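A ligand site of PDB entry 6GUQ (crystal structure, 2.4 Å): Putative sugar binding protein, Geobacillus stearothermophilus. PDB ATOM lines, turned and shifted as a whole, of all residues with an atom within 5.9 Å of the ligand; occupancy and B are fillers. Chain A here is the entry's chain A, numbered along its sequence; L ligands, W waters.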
ATOM      1  N   GLU A  38      18.977 -20.400  14.899  1.00  0.00           N
ATOM      2  CA  GLU A  38      18.498 -20.207  13.524  1.00  0.00           C
ATOM      3  C   GLU A  38      17.143 -20.877  13.296  1.00  0.00           C
ATOM      4  O   GLU A  38      16.336 -20.394  12.487  1.00  0.00           O
ATOM      5  CB  GLU A  38      19.519 -20.741  12.513  1.00  0.00           C
ATOM      6  CG  GLU A  38      19.208 -20.408  11.027  1.00  0.00           C
ATOM      7  CD  GLU A  38      20.424 -20.477  10.089  1.00  0.00           C
ATOM      8  OE1 GLU A  38      21.507 -20.928  10.525  1.00  0.00           O
ATOM      9  OE2 GLU A  38      20.303 -20.108   8.896  1.00  0.00           O
ATOM     10  N   ASN A  42      16.131 -27.634  15.137  1.00  0.00           N
ATOM     11  CA  ASN A  42      17.275 -28.115  14.377  1.00  0.00           C
ATOM     12  C   ASN A  42      18.275 -28.867  15.274  1.00  0.00           C
ATOM     13  O   ASN A  42      18.598 -28.415  16.377  1.00  0.00           O
ATOM     14  CB  ASN A  42      17.953 -26.936  13.675  1.00  0.00           C
ATOM     15  CG  ASN A  42      19.178 -27.343  12.888  1.00  0.00           C
ATOM     16  OD1 ASN A  42      20.244 -27.597  13.467  1.00  0.00           O
ATOM     17  ND2 ASN A  42      19.043 -27.407  11.563  1.00  0.00           N
ATOM     18  N   TYR A  44      21.493 -29.504  15.294  1.00  0.00           N
ATOM     19  CA  TYR A  44      22.741 -28.858  15.702  1.00  0.00           C
ATOM     20  C   TYR A  44      22.500 -27.828  16.802  1.00  0.00           C
ATOM     21  O   TYR A  44      23.235 -27.792  17.804  1.00  0.00           O
ATOM     22  CB  TYR A  44      23.381 -28.212  14.455  1.00  0.00           C
ATOM     23  CG  TYR A  44      24.504 -27.213  14.704  1.00  0.00           C
ATOM     24  CD1 TYR A  44      24.223 -25.875  14.969  1.00  0.00           C
ATOM     25  CD2 TYR A  44      25.844 -27.594  14.618  1.00  0.00           C
ATOM     26  CE1 TYR A  44      25.231 -24.957  15.187  1.00  0.00           C
ATOM     27  CE2 TYR A  44      26.876 -26.661  14.837  1.00  0.00           C
ATOM     28  CZ  TYR A  44      26.554 -25.351  15.124  1.00  0.00           C
ATOM     29  OH  TYR A  44      27.540 -24.410  15.338  1.00  0.00           O
ATOM     30  N   TRP A  45      21.454 -27.018  16.675  1.00  0.00           N
ATOM     31  CA  TRP A  45      21.133 -26.014  17.675  1.00  0.00           C
ATOM     32  C   TRP A  45      20.741 -26.637  19.013  1.00  0.00           C
ATOM     33  O   TRP A  45      20.983 -26.034  20.061  1.00  0.00           O
ATOM     34  CB  TRP A  45      20.023 -25.101  17.143  1.00  0.00           C
ATOM     35  CG  TRP A  45      20.618 -24.141  16.209  1.00  0.00           C
ATOM     36  CD1 TRP A  45      20.544 -24.154  14.859  1.00  0.00           C
ATOM     37  CD2 TRP A  45      21.481 -23.045  16.554  1.00  0.00           C
ATOM     38  NE1 TRP A  45      21.282 -23.114  14.330  1.00  0.00           N
ATOM     39  CE2 TRP A  45      21.854 -22.413  15.353  1.00  0.00           C
ATOM     40  CE3 TRP A  45      21.949 -22.525  17.765  1.00  0.00           C
ATOM     41  CZ2 TRP A  45      22.677 -21.297  15.330  1.00  0.00           C
ATOM     42  CZ3 TRP A  45      22.767 -21.415  17.736  1.00  0.00           C
ATOM     43  CH2 TRP A  45      23.124 -20.809  16.524  1.00  0.00           C
ATOM     44  N   GLN A  94      22.886 -15.375  16.440  1.00  0.00           N
ATOM     45  CA  GLN A  94      23.624 -15.289  15.189  1.00  0.00           C
ATOM     46  C   GLN A  94      23.543 -13.874  14.617  1.00  0.00           C
ATOM     47  O   GLN A  94      22.539 -13.179  14.773  1.00  0.00           O
ATOM     48  CB  GLN A  94      23.061 -16.235  14.127  1.00  0.00           C
ATOM     49  CG  GLN A  94      23.458 -17.690  14.184  1.00  0.00           C
ATOM     50  CD  GLN A  94      22.546 -18.546  13.270  1.00  0.00           C
ATOM     51  OE1 GLN A  94      21.315 -18.485  13.381  1.00  0.00           O
ATOM     52  NE2 GLN A  94      23.140 -19.324  12.367  1.00  0.00           N
ATOM     53  N   ASP A 119      28.036 -18.521  16.616  1.00  0.00           N
ATOM     54  CA  ASP A 119      27.976 -19.403  15.439  1.00  0.00           C
ATOM     55  C   ASP A 119      28.196 -18.635  14.128  1.00  0.00           C
ATOM     56  O   ASP A 119      28.928 -19.107  13.233  1.00  0.00           O
ATOM     57  CB  ASP A 119      26.640 -20.162  15.444  1.00  0.00           C
ATOM     58  CG  ASP A 119      26.384 -20.946  14.160  1.00  0.00           C
ATOM     59  OD1 ASP A 119      25.848 -20.355  13.197  1.00  0.00           O
ATOM     60  OD2 ASP A 119      26.697 -22.159  14.120  1.00  0.00           O
ATOM     61  N   THR A 120      27.588 -17.470  13.998  1.00  0.00           N
ATOM     62  CA  THR A 120      27.734 -16.600  12.829  1.00  0.00           C
ATOM     63  C   THR A 120      27.932 -15.179  13.329  1.00  0.00           C
ATOM     64  O   THR A 120      27.072 -14.648  14.044  1.00  0.00           O
ATOM     65  CB  THR A 120      26.502 -16.694  11.918  1.00  0.00           C
ATOM     66  OG1 THR A 120      26.218 -18.067  11.626  1.00  0.00           O
ATOM     67  CG2 THR A 120      26.730 -15.925  10.630  1.00  0.00           C
ATOM     68  N   ASN A 135      34.433 -19.134  10.269  1.00  0.00           N
ATOM     69  CA  ASN A 135      33.717 -19.660   9.158  1.00  0.00           C
ATOM     70  C   ASN A 135      34.452 -19.730   7.861  1.00  0.00           C
ATOM     71  O   ASN A 135      34.295 -20.660   7.182  1.00  0.00           O
ATOM     72  CB  ASN A 135      32.363 -18.997   9.023  1.00  0.00           C
ATOM     73  CG  ASN A 135      31.392 -19.451  10.076  1.00  0.00           C
ATOM     74  OD1 ASN A 135      31.278 -20.592  10.339  1.00  0.00           O
ATOM     75  ND2 ASN A 135      30.688 -18.540  10.654  1.00  0.00           N
ATOM     76  N   HIS A 167      27.583 -16.911   7.438  1.00  0.00           N
ATOM     77  CA  HIS A 167      28.490 -18.028   7.647  1.00  0.00           C
ATOM     78  C   HIS A 167      28.515 -18.955   6.449  1.00  0.00           C
ATOM     79  O   HIS A 167      29.585 -19.473   6.091  1.00  0.00           O
ATOM     80  CB  HIS A 167      28.131 -18.799   8.938  1.00  0.00           C
ATOM     81  CG  HIS A 167      26.723 -19.332   8.997  1.00  0.00           C
ATOM     82  ND1 HIS A 167      25.648 -18.732   8.376  1.00  0.00           N
ATOM     83  CD2 HIS A 167      26.208 -20.382   9.689  1.00  0.00           C
ATOM     84  CE1 HIS A 167      24.552 -19.411   8.649  1.00  0.00           C
ATOM     85  NE2 HIS A 167      24.861 -20.409   9.456  1.00  0.00           N
ATOM     86  N   GLN A 168      27.358 -19.120   5.793  1.00  0.00           N
ATOM     87  CA  GLN A 168      27.286 -19.955   4.600  1.00  0.00           C
ATOM     88  C   GLN A 168      28.142 -19.375   3.479  1.00  0.00           C
ATOM     89  O   GLN A 168      28.927 -20.088   2.846  1.00  0.00           O
ATOM     90  CB  GLN A 168      25.834 -20.096   4.152  1.00  0.00           C
ATOM     91  CG  GLN A 168      24.957 -20.771   5.162  1.00  0.00           C
ATOM     92  CD  GLN A 168      25.485 -22.135   5.551  1.00  0.00           C
ATOM     93  OE1 GLN A 168      25.335 -23.114   4.804  1.00  0.00           O
ATOM     94  NE2 GLN A 168      26.114 -22.220   6.709  1.00  0.00           N
ATOM     95  N   ARG A 171      31.831 -20.021   4.353  1.00  0.00           N
ATOM     96  CA  ARG A 171      32.223 -21.407   4.080  1.00  0.00           C
ATOM     97  C   ARG A 171      32.300 -21.688   2.585  1.00  0.00           C
ATOM     98  O   ARG A 171      33.132 -22.493   2.139  1.00  0.00           O
ATOM     99  CB  ARG A 171      31.262 -22.375   4.774  1.00  0.00           C
ATOM    100  CG  ARG A 171      31.290 -22.281   6.293  1.00  0.00           C
ATOM    101  CD  ARG A 171      30.106 -23.000   6.920  1.00  0.00           C
ATOM    102  NE  ARG A 171      29.933 -22.621   8.313  1.00  0.00           N
ATOM    103  CZ  ARG A 171      29.116 -23.223   9.179  1.00  0.00           C
ATOM    104  NH1 ARG A 171      28.375 -24.245   8.808  1.00  0.00           N
ATOM    105  NH2 ARG A 171      29.029 -22.800  10.436  1.00  0.00           N
ATOM    106  N   ILE A 195      18.556 -25.421   4.997  1.00  0.00           N
ATOM    107  CA  ILE A 195      18.956 -26.249   6.142  1.00  0.00           C
ATOM    108  C   ILE A 195      17.943 -27.319   6.546  1.00  0.00           C
ATOM    109  O   ILE A 195      17.760 -27.596   7.738  1.00  0.00           O
ATOM    110  CB  ILE A 195      19.365 -25.358   7.352  1.00  0.00           C
ATOM    111  CG1 ILE A 195      18.215 -24.543   7.946  1.00  0.00           C
ATOM    112  CG2 ILE A 195      20.531 -24.419   6.981  1.00  0.00           C
ATOM    113  CD1 ILE A 195      18.385 -24.284   9.395  1.00  0.00           C
ATOM    114  N   THR A 220      27.636 -27.336   3.252  1.00  0.00           N
ATOM    115  CA  THR A 220      28.173 -26.294   4.138  1.00  0.00           C
ATOM    116  C   THR A 220      27.384 -26.108   5.434  1.00  0.00           C
ATOM    117  O   THR A 220      27.785 -25.261   6.250  1.00  0.00           O
ATOM    118  CB  THR A 220      28.284 -24.953   3.380  1.00  0.00           C
ATOM    119  OG1 THR A 220      26.998 -24.348   3.217  1.00  0.00           O
ATOM    120  CG2 THR A 220      28.935 -25.129   2.037  1.00  0.00           C
ATOM    121  N   SER A 221      26.326 -26.875   5.680  1.00  0.00           N
ATOM    122  CA  SER A 221      25.609 -26.819   6.947  1.00  0.00           C
ATOM    123  C   SER A 221      25.295 -28.231   7.434  1.00  0.00           C
ATOM    124  O   SER A 221      25.525 -29.225   6.735  1.00  0.00           O
ATOM    125  CB  SER A 221      24.339 -25.967   6.820  1.00  0.00           C
ATOM    126  OG  SER A 221      23.389 -26.557   5.948  1.00  0.00           O
ATOM    127  N   ALA A 222      24.738 -28.327   8.644  1.00  0.00           N
ATOM    128  CA  ALA A 222      24.768 -29.585   9.400  1.00  0.00           C
ATOM    129  C   ALA A 222      24.007 -30.733   8.723  1.00  0.00           C
ATOM    130  O   ALA A 222      24.356 -31.912   8.922  1.00  0.00           O
ATOM    131  CB  ALA A 222      24.233 -29.360  10.814  1.00  0.00           C
ATOM    132  N   LEU A 223      22.968 -30.445   7.952  1.00  0.00           N
ATOM    133  CA  LEU A 223      22.122 -31.499   7.387  1.00  0.00           C
ATOM    134  C   LEU A 223      22.343 -31.720   5.890  1.00  0.00           C
ATOM    135  O   LEU A 223      21.590 -32.486   5.262  1.00  0.00           O
ATOM    136  CB  LEU A 223      20.653 -31.162   7.639  1.00  0.00           C
ATOM    137  CG  LEU A 223      20.209 -31.050   9.098  1.00  0.00           C
ATOM    138  CD1 LEU A 223      18.819 -30.383   9.202  1.00  0.00           C
ATOM    139  CD2 LEU A 223      20.211 -32.419   9.744  1.00  0.00           C
ATOM    140  N   PHE A 246      29.460 -30.924   6.713  1.00  0.00           N
ATOM    141  CA  PHE A 246      29.740 -30.189   7.934  1.00  0.00           C
ATOM    142  C   PHE A 246      29.170 -30.921   9.145  1.00  0.00           C
ATOM    143  O   PHE A 246      28.176 -31.648   9.041  1.00  0.00           O
ATOM    144  CB  PHE A 246      29.148 -28.768   7.891  1.00  0.00           C
ATOM    145  CG  PHE A 246      30.185 -27.681   7.705  1.00  0.00           C
ATOM    146  CD1 PHE A 246      30.771 -27.482   6.464  1.00  0.00           C
ATOM    147  CD2 PHE A 246      30.561 -26.865   8.780  1.00  0.00           C
ATOM    148  CE1 PHE A 246      31.737 -26.471   6.284  1.00  0.00           C
ATOM    149  CE2 PHE A 246      31.529 -25.857   8.617  1.00  0.00           C
ATOM    150  CZ  PHE A 246      32.116 -25.658   7.376  1.00  0.00           C
ATOM    151  N   ASP A 247      29.835 -30.722  10.281  1.00  0.00           N
ATOM    152  CA  ASP A 247      29.351 -31.137  11.599  1.00  0.00           C
ATOM    153  C   ASP A 247      29.321 -32.658  11.780  1.00  0.00           C
ATOM    154  O   ASP A 247      29.656 -33.416  10.846  1.00  0.00           O
ATOM    155  CB  ASP A 247      27.985 -30.520  11.874  1.00  0.00           C
ATOM    156  CG  ASP A 247      28.045 -28.989  11.854  1.00  0.00           C
ATOM    157  OD1 ASP A 247      28.835 -28.417  12.675  1.00  0.00           O
ATOM    158  OD2 ASP A 247      27.333 -28.375  11.021  1.00  0.00           O
ATOM    159  N   GLN A 267      32.587 -29.052  14.108  1.00  0.00           N
ATOM    160  CA  GLN A 267      32.341 -27.861  14.919  1.00  0.00           C
ATOM    161  C   GLN A 267      32.113 -28.269  16.365  1.00  0.00           C
ATOM    162  O   GLN A 267      31.983 -29.455  16.690  1.00  0.00           O
ATOM    163  CB  GLN A 267      31.145 -27.041  14.434  1.00  0.00           C
ATOM    164  CG  GLN A 267      31.272 -26.495  13.047  1.00  0.00           C
ATOM    165  CD  GLN A 267      30.278 -25.393  12.748  1.00  0.00           C
ATOM    166  OE1 GLN A 267      30.592 -24.209  12.869  1.00  0.00           O
ATOM    167  NE2 GLN A 267      29.057 -25.785  12.377  1.00  0.00           N
HETATM  168  C1  LIG L   1      25.612 -24.055  11.157  1.00  0.00           C
HETATM  169  C2  LIG L   1      24.364 -23.445  11.692  1.00  0.00           C
HETATM  170  C3  LIG L   1      23.200 -23.891  10.875  1.00  0.00           C
HETATM  171  C4  LIG L   1      23.058 -25.408  10.895  1.00  0.00           C
HETATM  172  C5  LIG L   1      21.936 -25.765   9.964  1.00  0.00           C
HETATM  173  C6  LIG L   1      25.526 -25.564  11.059  1.00  0.00           C
HETATM  174  O1  LIG L   1      26.562 -26.014  10.290  1.00  0.00           O
HETATM  175  O2  LIG L   1      26.777 -23.747  11.939  1.00  0.00           O
HETATM  176  O3  LIG L   1      24.420 -22.020  11.484  1.00  0.00           O
HETATM  177  O4  LIG L   1      21.967 -23.369  11.355  1.00  0.00           O
HETATM  178  O5  LIG L   1      24.278 -26.043  10.400  1.00  0.00           O
HETATM  179  O6  LIG L   1      21.656 -27.118  10.133  1.00  0.00           O
HETATM  180  O   HOH W   1      21.640 -27.944   7.280  1.00  0.00           O
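Water W1 lies within hydrogen-bond range of OG of Ser 221, N of Leu 223, O6 of the ligand and N of Ala 222.
Tyr 44 touches the ligand. Ile 195 touches the ligand (CG2 to C5, 3.6 Å). Ser 221 touches the ligand. Within 4 Å of the ligand: Glu 38, Asn 42, Tyr 44, Trp 45, Gln 94, Asp 119, His 167, Arg 171, Ile 195, Ser 221, Ala 222, Asp 247 and Gln 267.
OD2 of Asp 247 sits at hydrogen-bond distance from O1 of the ligand. An oxygen (O4) of the ligand is in hydrogen-bond range of the side-chain carboxylate (OE1) of Glu 38, at 2.6 Å. An oxygen (O3) of the ligand is in hydrogen-bond range of a ring nitrogen (NE2) of His 167, at 2.6 Å. The side-chain carboxylate (OD2) of Asp 119 lies within hydrogen-bond range of an oxygen (O2) of the ligand (2.7 Å). O2 of the ligand is in hydrogen-bond range of NH2 of Arg 171, 2.9 Å away. The backbone NH (N) of Ala 222 sits at hydrogen-bond distance from an oxygen (O5) of the ligand. The side-chain amide nitrogen (ND2) of Asn 42 lies within hydrogen-bond range of an oxygen (O6) of the ligand (3.0 Å). The indole nitrogen (NE1) of Trp 45 sits at hydrogen-bond distance from an oxygen (O4) of the ligand (3.1 Å). The side-chain amide nitrogen (NE2) of Gln 267 lies within hydrogen-bond range of an oxygen (O2) of the ligand, 3.1 Å away. O3 of the ligand is in hydrogen-bond range of NE2 of Gln 94 (3.1 Å).
NE2 of Gln 94 sits at hydrogen-bond distance from OE1 of Glu 38 (2.9 Å). A ring nitrogen (ND1) of His 167 lies close to the side-chain hydroxyl (OG1) of Thr 120. The side-chain amide nitrogen of Gln 94 is in hydrogen-bond range of the side-chain carboxylate of Asp 119 (3.0 Å). OH of Tyr 44 lies within hydrogen-bond range of OD2 of Asp 119 (2.7 Å). The side-chain hydroxyl of Thr 120 is in hydrogen-bond range of the side-chain carboxylate of Asp 119 (2.8 Å). The guanidinium group of Arg 171 sits at hydrogen-bond distance from the side-chain amide oxygen of Gln 267 (3.2 Å). The guanidinium group of Arg 171 lies within hydrogen-bond range of the side-chain amide oxygen of Asn 135, 3.2 Å away. NE2 of Gln 94 sits at hydrogen-bond distance from OG1 of Thr 120 (3.4 Å).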
